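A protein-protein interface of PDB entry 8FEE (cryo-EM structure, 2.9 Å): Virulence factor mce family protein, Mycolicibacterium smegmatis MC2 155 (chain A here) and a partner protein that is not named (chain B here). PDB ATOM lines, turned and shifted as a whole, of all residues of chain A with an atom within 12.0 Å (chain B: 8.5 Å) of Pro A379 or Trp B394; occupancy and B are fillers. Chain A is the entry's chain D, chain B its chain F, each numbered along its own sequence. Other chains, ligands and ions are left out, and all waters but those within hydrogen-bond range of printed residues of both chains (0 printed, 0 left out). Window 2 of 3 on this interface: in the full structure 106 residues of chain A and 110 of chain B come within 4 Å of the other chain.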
ATOM      1  N   VAL A 329      19.151 -24.747   1.576  1.00  0.00           N
ATOM      2  CA  VAL A 329      17.929 -25.413   2.007  1.00  0.00           C
ATOM      3  C   VAL A 329      17.422 -24.785   3.299  1.00  0.00           C
ATOM      4  O   VAL A 329      16.523 -25.317   3.950  1.00  0.00           O
ATOM      5  CB  VAL A 329      18.149 -26.925   2.190  1.00  0.00           C
ATOM      6  CG1 VAL A 329      18.573 -27.562   0.878  1.00  0.00           C
ATOM      7  CG2 VAL A 329      19.183 -27.182   3.271  1.00  0.00           C
ATOM      8  N   PHE A 375       9.606 -30.145  12.716  1.00  0.00           N
ATOM      9  CA  PHE A 375       9.163 -30.314  11.338  1.00  0.00           C
ATOM     10  C   PHE A 375      10.349 -30.344  10.378  1.00  0.00           C
ATOM     11  O   PHE A 375      11.405 -29.785  10.669  1.00  0.00           O
ATOM     12  CB  PHE A 375       8.183 -29.202  10.950  1.00  0.00           C
ATOM     13  CG  PHE A 375       8.734 -27.811  11.116  1.00  0.00           C
ATOM     14  CD1 PHE A 375       9.415 -27.190  10.082  1.00  0.00           C
ATOM     15  CD2 PHE A 375       8.553 -27.119  12.302  1.00  0.00           C
ATOM     16  CE1 PHE A 375       9.917 -25.912  10.232  1.00  0.00           C
ATOM     17  CE2 PHE A 375       9.052 -25.841  12.458  1.00  0.00           C
ATOM     18  CZ  PHE A 375       9.735 -25.237  11.421  1.00  0.00           C
ATOM     19  N   ASN A 376      10.164 -31.003   9.232  1.00  0.00           N
ATOM     20  CA  ASN A 376      11.259 -31.149   8.276  1.00  0.00           C
ATOM     21  C   ASN A 376      11.576 -29.828   7.585  1.00  0.00           C
ATOM     22  O   ASN A 376      12.746 -29.445   7.469  1.00  0.00           O
ATOM     23  CB  ASN A 376      10.918 -32.228   7.249  1.00  0.00           C
ATOM     24  CG  ASN A 376      10.846 -33.612   7.862  1.00  0.00           C
ATOM     25  OD1 ASN A 376      11.463 -33.878   8.892  1.00  0.00           O
ATOM     26  ND2 ASN A 376      10.093 -34.502   7.227  1.00  0.00           N
ATOM     27  N   TYR A 377      10.552 -29.116   7.123  1.00  0.00           N
ATOM     28  CA  TYR A 377      10.755 -27.869   6.396  1.00  0.00           C
ATOM     29  C   TYR A 377       9.474 -27.047   6.466  1.00  0.00           C
ATOM     30  O   TYR A 377       8.476 -27.460   7.062  1.00  0.00           O
ATOM     31  CB  TYR A 377      11.166 -28.131   4.942  1.00  0.00           C
ATOM     32  CG  TYR A 377      10.312 -29.163   4.237  1.00  0.00           C
ATOM     33  CD1 TYR A 377       9.124 -28.803   3.616  1.00  0.00           C
ATOM     34  CD2 TYR A 377      10.700 -30.492   4.184  1.00  0.00           C
ATOM     35  CE1 TYR A 377       8.341 -29.742   2.972  1.00  0.00           C
ATOM     36  CE2 TYR A 377       9.924 -31.437   3.543  1.00  0.00           C
ATOM     37  CZ  TYR A 377       8.748 -31.056   2.937  1.00  0.00           C
ATOM     38  OH  TYR A 377       7.975 -31.995   2.294  1.00  0.00           O
ATOM     39  N   LEU A 378       9.515 -25.870   5.844  1.00  0.00           N
ATOM     40  CA  LEU A 378       8.385 -24.951   5.833  1.00  0.00           C
ATOM     41  C   LEU A 378       7.319 -25.431   4.849  1.00  0.00           C
ATOM     42  O   LEU A 378       7.649 -25.951   3.781  1.00  0.00           O
ATOM     43  CB  LEU A 378       8.843 -23.545   5.456  1.00  0.00           C
ATOM     44  CG  LEU A 378       9.719 -22.835   6.488  1.00  0.00           C
ATOM     45  CD1 LEU A 378      10.239 -21.518   5.938  1.00  0.00           C
ATOM     46  CD2 LEU A 378       8.940 -22.613   7.772  1.00  0.00           C
ATOM     47  N   PRO A 379       6.036 -25.274   5.190  1.00  0.00           N
ATOM     48  CA  PRO A 379       4.970 -25.726   4.280  1.00  0.00           C
ATOM     49  C   PRO A 379       4.950 -25.007   2.943  1.00  0.00           C
ATOM     50  O   PRO A 379       4.414 -25.556   1.973  1.00  0.00           O
ATOM     51  CB  PRO A 379       3.687 -25.446   5.075  1.00  0.00           C
ATOM     52  CG  PRO A 379       4.119 -25.385   6.495  1.00  0.00           C
ATOM     53  CD  PRO A 379       5.503 -24.812   6.481  1.00  0.00           C
ATOM     54  N   PHE A 380       5.507 -23.806   2.855  1.00  0.00           N
ATOM     55  CA  PHE A 380       5.402 -22.980   1.664  1.00  0.00           C
ATOM     56  C   PHE A 380       6.772 -22.777   1.032  1.00  0.00           C
ATOM     57  O   PHE A 380       7.799 -22.773   1.717  1.00  0.00           O
ATOM     58  CB  PHE A 380       4.770 -21.619   1.988  1.00  0.00           C
ATOM     59  CG  PHE A 380       5.228 -21.033   3.294  1.00  0.00           C
ATOM     60  CD1 PHE A 380       6.398 -20.297   3.365  1.00  0.00           C
ATOM     61  CD2 PHE A 380       4.483 -21.214   4.449  1.00  0.00           C
ATOM     62  CE1 PHE A 380       6.821 -19.756   4.565  1.00  0.00           C
ATOM     63  CE2 PHE A 380       4.901 -20.677   5.651  1.00  0.00           C
ATOM     64  CZ  PHE A 380       6.071 -19.947   5.709  1.00  0.00           C
ATOM     65  N   GLY A 381       6.771 -22.609  -0.289  1.00  0.00           N
ATOM     66  CA  GLY A 381       7.996 -22.393  -1.027  1.00  0.00           C
ATOM     67  C   GLY A 381       7.777 -21.357  -2.109  1.00  0.00           C
ATOM     68  O   GLY A 381       6.648 -21.093  -2.526  1.00  0.00           O
ATOM     69  N   MET A 382       8.881 -20.766  -2.561  1.00  0.00           N
ATOM     70  CA  MET A 382       8.807 -19.705  -3.551  1.00  0.00           C
ATOM     71  C   MET A 382       9.973 -19.822  -4.523  1.00  0.00           C
ATOM     72  O   MET A 382      11.025 -20.379  -4.204  1.00  0.00           O
ATOM     73  CB  MET A 382       8.801 -18.323  -2.878  1.00  0.00           C
ATOM     74  CG  MET A 382       8.258 -17.200  -3.747  1.00  0.00           C
ATOM     75  SD  MET A 382       7.769 -15.756  -2.785  1.00  0.00           S
ATOM     76  CE  MET A 382       6.595 -14.989  -3.901  1.00  0.00           C
ATOM     77  N   ASN A 383       9.764 -19.287  -5.727  1.00  0.00           N
ATOM     78  CA  ASN A 383      10.818 -19.165  -6.733  1.00  0.00           C
ATOM     79  C   ASN A 383      10.461 -17.957  -7.595  1.00  0.00           C
ATOM     80  O   ASN A 383       9.583 -18.049  -8.457  1.00  0.00           O
ATOM     81  CB  ASN A 383      10.945 -20.434  -7.564  1.00  0.00           C
ATOM     82  CG  ASN A 383      12.077 -20.361  -8.571  1.00  0.00           C
ATOM     83  OD1 ASN A 383      11.864 -20.034  -9.738  1.00  0.00           O
ATOM     84  ND2 ASN A 383      13.287 -20.665  -8.122  1.00  0.00           N
ATOM     85  N   ILE B 315      13.301 -19.638  -1.977  1.00  0.00           N
ATOM     86  CA  ILE B 315      13.335 -20.345  -0.702  1.00  0.00           C
ATOM     87  C   ILE B 315      12.407 -21.549  -0.788  1.00  0.00           C
ATOM     88  O   ILE B 315      11.217 -21.407  -1.098  1.00  0.00           O
ATOM     89  CB  ILE B 315      12.951 -19.423   0.466  1.00  0.00           C
ATOM     90  CG1 ILE B 315      11.753 -18.545   0.095  1.00  0.00           C
ATOM     91  CG2 ILE B 315      14.135 -18.563   0.873  1.00  0.00           C
ATOM     92  CD1 ILE B 315      11.324 -17.602   1.197  1.00  0.00           C
ATOM     93  N   ASN B 316      12.962 -22.733  -0.517  1.00  0.00           N
ATOM     94  CA  ASN B 316      12.212 -23.991  -0.464  1.00  0.00           C
ATOM     95  C   ASN B 316      11.429 -24.253  -1.749  1.00  0.00           C
ATOM     96  O   ASN B 316      10.258 -24.636  -1.718  1.00  0.00           O
ATOM     97  CB  ASN B 316      11.281 -24.022   0.750  1.00  0.00           C
ATOM     98  CG  ASN B 316      11.946 -24.598   1.980  1.00  0.00           C
ATOM     99  OD1 ASN B 316      13.169 -24.575   2.105  1.00  0.00           O
ATOM    100  ND2 ASN B 316      11.140 -25.122   2.896  1.00  0.00           N
ATOM    101  N   PRO B 319      11.643 -28.904  -1.794  1.00  0.00           N
ATOM    102  CA  PRO B 319      12.012 -29.256  -0.425  1.00  0.00           C
ATOM    103  C   PRO B 319      12.821 -30.538  -0.417  1.00  0.00           C
ATOM    104  O   PRO B 319      12.379 -31.563  -0.955  1.00  0.00           O
ATOM    105  CB  PRO B 319      10.656 -29.438   0.271  1.00  0.00           C
ATOM    106  CG  PRO B 319       9.738 -29.852  -0.822  1.00  0.00           C
ATOM    107  CD  PRO B 319      10.221 -29.165  -2.073  1.00  0.00           C
ATOM    108  N   PRO B 320      14.021 -30.518   0.160  1.00  0.00           N
ATOM    109  CA  PRO B 320      14.835 -31.738   0.190  1.00  0.00           C
ATOM    110  C   PRO B 320      14.170 -32.852   0.984  1.00  0.00           C
ATOM    111  O   PRO B 320      13.470 -32.615   1.971  1.00  0.00           O
ATOM    112  CB  PRO B 320      16.135 -31.275   0.857  1.00  0.00           C
ATOM    113  CG  PRO B 320      15.732 -30.087   1.669  1.00  0.00           C
ATOM    114  CD  PRO B 320      14.676 -29.400   0.858  1.00  0.00           C
ATOM    115  N   LEU B 322      14.128 -36.245   3.331  1.00  0.00           N
ATOM    116  CA  LEU B 322      14.822 -36.929   4.413  1.00  0.00           C
ATOM    117  C   LEU B 322      14.487 -38.414   4.490  1.00  0.00           C
ATOM    118  O   LEU B 322      14.846 -39.068   5.474  1.00  0.00           O
ATOM    119  CB  LEU B 322      14.509 -36.252   5.749  1.00  0.00           C
ATOM    120  CG  LEU B 322      14.772 -34.746   5.822  1.00  0.00           C
ATOM    121  CD1 LEU B 322      14.485 -34.219   7.219  1.00  0.00           C
ATOM    122  CD2 LEU B 322      16.198 -34.425   5.411  1.00  0.00           C
ATOM    123  N   THR B 391       6.653 -41.432   1.623  1.00  0.00           N
ATOM    124  CA  THR B 391       6.551 -40.070   1.120  1.00  0.00           C
ATOM    125  C   THR B 391       7.164 -39.102   2.122  1.00  0.00           C
ATOM    126  O   THR B 391       6.979 -39.244   3.333  1.00  0.00           O
ATOM    127  CB  THR B 391       5.092 -39.698   0.859  1.00  0.00           C
ATOM    128  OG1 THR B 391       4.371 -39.683   2.096  1.00  0.00           O
ATOM    129  CG2 THR B 391       4.448 -40.701  -0.085  1.00  0.00           C
ATOM    130  N   ASN B 392       7.899 -38.117   1.612  1.00  0.00           N
ATOM    131  CA  ASN B 392       8.597 -37.152   2.453  1.00  0.00           C
ATOM    132  C   ASN B 392       7.626 -36.113   3.005  1.00  0.00           C
ATOM    133  O   ASN B 392       7.093 -35.295   2.246  1.00  0.00           O
ATOM    134  CB  ASN B 392       9.715 -36.479   1.656  1.00  0.00           C
ATOM    135  CG  ASN B 392      10.230 -35.223   2.319  1.00  0.00           C
ATOM    136  OD1 ASN B 392       9.843 -34.115   1.953  1.00  0.00           O
ATOM    137  ND2 ASN B 392      11.108 -35.386   3.299  1.00  0.00           N
ATOM    138  N   PRO B 393       7.371 -36.112   4.309  1.00  0.00           N
ATOM    139  CA  PRO B 393       6.403 -35.182   4.888  1.00  0.00           C
ATOM    140  C   PRO B 393       7.064 -33.889   5.354  1.00  0.00           C
ATOM    141  O   PRO B 393       8.288 -33.782   5.456  1.00  0.00           O
ATOM    142  CB  PRO B 393       5.841 -35.966   6.088  1.00  0.00           C
ATOM    143  CG  PRO B 393       6.690 -37.239   6.196  1.00  0.00           C
ATOM    144  CD  PRO B 393       7.889 -37.033   5.329  1.00  0.00           C
ATOM    145  N   TRP B 394       6.220 -32.898   5.633  1.00  0.00           N
ATOM    146  CA  TRP B 394       6.687 -31.613   6.133  1.00  0.00           C
ATOM    147  C   TRP B 394       6.752 -31.553   7.652  1.00  0.00           C
ATOM    148  O   TRP B 394       7.332 -30.605   8.191  1.00  0.00           O
ATOM    149  CB  TRP B 394       5.778 -30.484   5.635  1.00  0.00           C
ATOM    150  CG  TRP B 394       4.524 -30.339   6.448  1.00  0.00           C
ATOM    151  CD1 TRP B 394       3.383 -31.077   6.333  1.00  0.00           C
ATOM    152  CD2 TRP B 394       4.292 -29.409   7.515  1.00  0.00           C
ATOM    153  NE1 TRP B 394       2.454 -30.661   7.253  1.00  0.00           N
ATOM    154  CE2 TRP B 394       2.987 -29.639   7.993  1.00  0.00           C
ATOM    155  CE3 TRP B 394       5.061 -28.406   8.111  1.00  0.00           C
ATOM    156  CZ2 TRP B 394       2.434 -28.901   9.037  1.00  0.00           C
ATOM    157  CZ3 TRP B 394       4.510 -27.674   9.148  1.00  0.00           C
ATOM    158  CH2 TRP B 394       3.208 -27.926   9.599  1.00  0.00           C
ATOM    159  N   TYR B 395       6.186 -32.535   8.351  1.00  0.00           N
ATOM    160  CA  TYR B 395       6.117 -32.489   9.807  1.00  0.00           C
ATOM    161  C   TYR B 395       6.855 -33.677  10.415  1.00  0.00           C
ATOM    162  O   TYR B 395       6.316 -34.389  11.268  1.00  0.00           O
ATOM    163  CB  TYR B 395       4.655 -32.443  10.267  1.00  0.00           C
ATOM    164  CG  TYR B 395       4.471 -32.185  11.749  1.00  0.00           C
ATOM    165  CD1 TYR B 395       4.957 -31.025  12.337  1.00  0.00           C
ATOM    166  CD2 TYR B 395       3.803 -33.099  12.556  1.00  0.00           C
ATOM    167  CE1 TYR B 395       4.793 -30.787  13.690  1.00  0.00           C
ATOM    168  CE2 TYR B 395       3.633 -32.870  13.907  1.00  0.00           C
ATOM    169  CZ  TYR B 395       4.128 -31.711  14.469  1.00  0.00           C
ATOM    170  OH  TYR B 395       3.959 -31.479  15.815  1.00  0.00           O
ATOM    171  N   GLY B 396       8.082 -33.913   9.965  1.00  0.00           N
ATOM    172  CA  GLY B 396       8.901 -34.929  10.587  1.00  0.00           C
ATOM    173  C   GLY B 396       8.422 -36.340  10.281  1.00  0.00           C
ATOM    174  O   GLY B 396       7.553 -36.576   9.440  1.00  0.00           O
ATOM    175  N   ASP B 397       9.009 -37.284  11.017  1.00  0.00           N
ATOM    176  CA  ASP B 397       8.769 -38.712  10.840  1.00  0.00           C
ATOM    177  C   ASP B 397       8.878 -39.174   9.383  1.00  0.00           C
ATOM    178  O   ASP B 397       7.944 -39.774   8.846  1.00  0.00           O
ATOM    179  CB  ASP B 397       7.409 -39.094  11.410  1.00  0.00           C
ATOM    180  CG  ASP B 397       7.237 -38.658  12.851  1.00  0.00           C
ATOM    181  OD1 ASP B 397       7.225 -37.436  13.106  1.00  0.00           O
ATOM    182  OD2 ASP B 397       7.110 -39.538  13.727  1.00  0.00           O
ATOM    183  N   PRO B 398      10.006 -38.907   8.709  1.00  0.00           N
ATOM    184  CA  PRO B 398      10.134 -39.360   7.315  1.00  0.00           C
ATOM    185  C   PRO B 398      10.247 -40.867   7.179  1.00  0.00           C
ATOM    186  O   PRO B 398       9.911 -41.391   6.109  1.00  0.00           O
ATOM    187  CB  PRO B 398      11.412 -38.662   6.834  1.00  0.00           C
ATOM    188  CG  PRO B 398      12.223 -38.521   8.058  1.00  0.00           C
ATOM    189  CD  PRO B 398      11.259 -38.290   9.188  1.00  0.00           C
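Val A329 touches Asn B316 (O to OD1, 3.9 Å). Val A329 touches Pro B320. Trp B394 touches Phe A375 (O to CB, 3.2 Å). CD1 of Leu B322 touches OD1 of Asn A376, at 3.5 Å. Tyr A377 touches Pro B393 (CE2 to O, 3.4 Å). Tyr A377 touches Trp B394 (O to O, 3.5 Å). CZ3 of Trp B394 touches CG of Pro A379 (3.5 Å). Asn B316 touches Phe A380 (CB to O, 3.8 Å). Ile B315 touches Gly A381. CA of Gly A381 touches O of Asn B316 (3.3 Å).
The side-chain amide nitrogen of Asn A376 is in hydrogen-bond range of the backbone carbonyl oxygen of Pro B393 (2.6 Å). The backbone carbonyl oxygen of Trp B394 sits at hydrogen-bond distance from the backbone NH of Asn A376 (3.0 Å). N of Gly B396 lies close to ND2 of Asn A376 (3.4 Å). The side-chain hydroxyl (OH) of Tyr A377 lies within hydrogen-bond range of the side-chain amide oxygen (OD1) of Asn B392 (2.8 Å). The backbone NH of Leu A378 lies close to the side-chain amide nitrogen of Asn B316, 3.4 Å away. N of Met A382 is in hydrogen-bond range of O of Ile B315 (2.8 Å).
Trp B394 touches just these residues of chain A: Phe A375, Asn A376, Tyr A377 and Pro A379. Of chain A, only Tyr A377 comes within 4 Å of Asn B392. Printed residues of chain A within 4 Å of Pro B393: Asn A376 and Tyr A377. Printed residues of chain B within 4 Å of Met A382: Ile B315 (2.8 Å). Of the printed residues of chain B, Val A329 touches Asn B316 (3.9 Å) and Pro B320 (3.9 Å). Thr B391 touches none of the printed residues of chain A. Pro B398 touches none of the printed residues of chain A. The nearest printed residue of chain A that does not touch Ile B315 is Phe A380 (4.6 Å).
ND2 of Asn B392 lies close to N of Leu B322, 3.1 Å away.
Along chain A the printed residues that touch a printed residue of chain B span positions 329 to 382. Of the 13 printed residues of chain B, 10 touch a printed residue of chain A. Among the printed residues, 19 pairs touch across the chains. Among the printed residues, no Asp or Glu carboxylate lies within 4 Å of a Lys or Arg side-chain nitrogen of the other chain.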
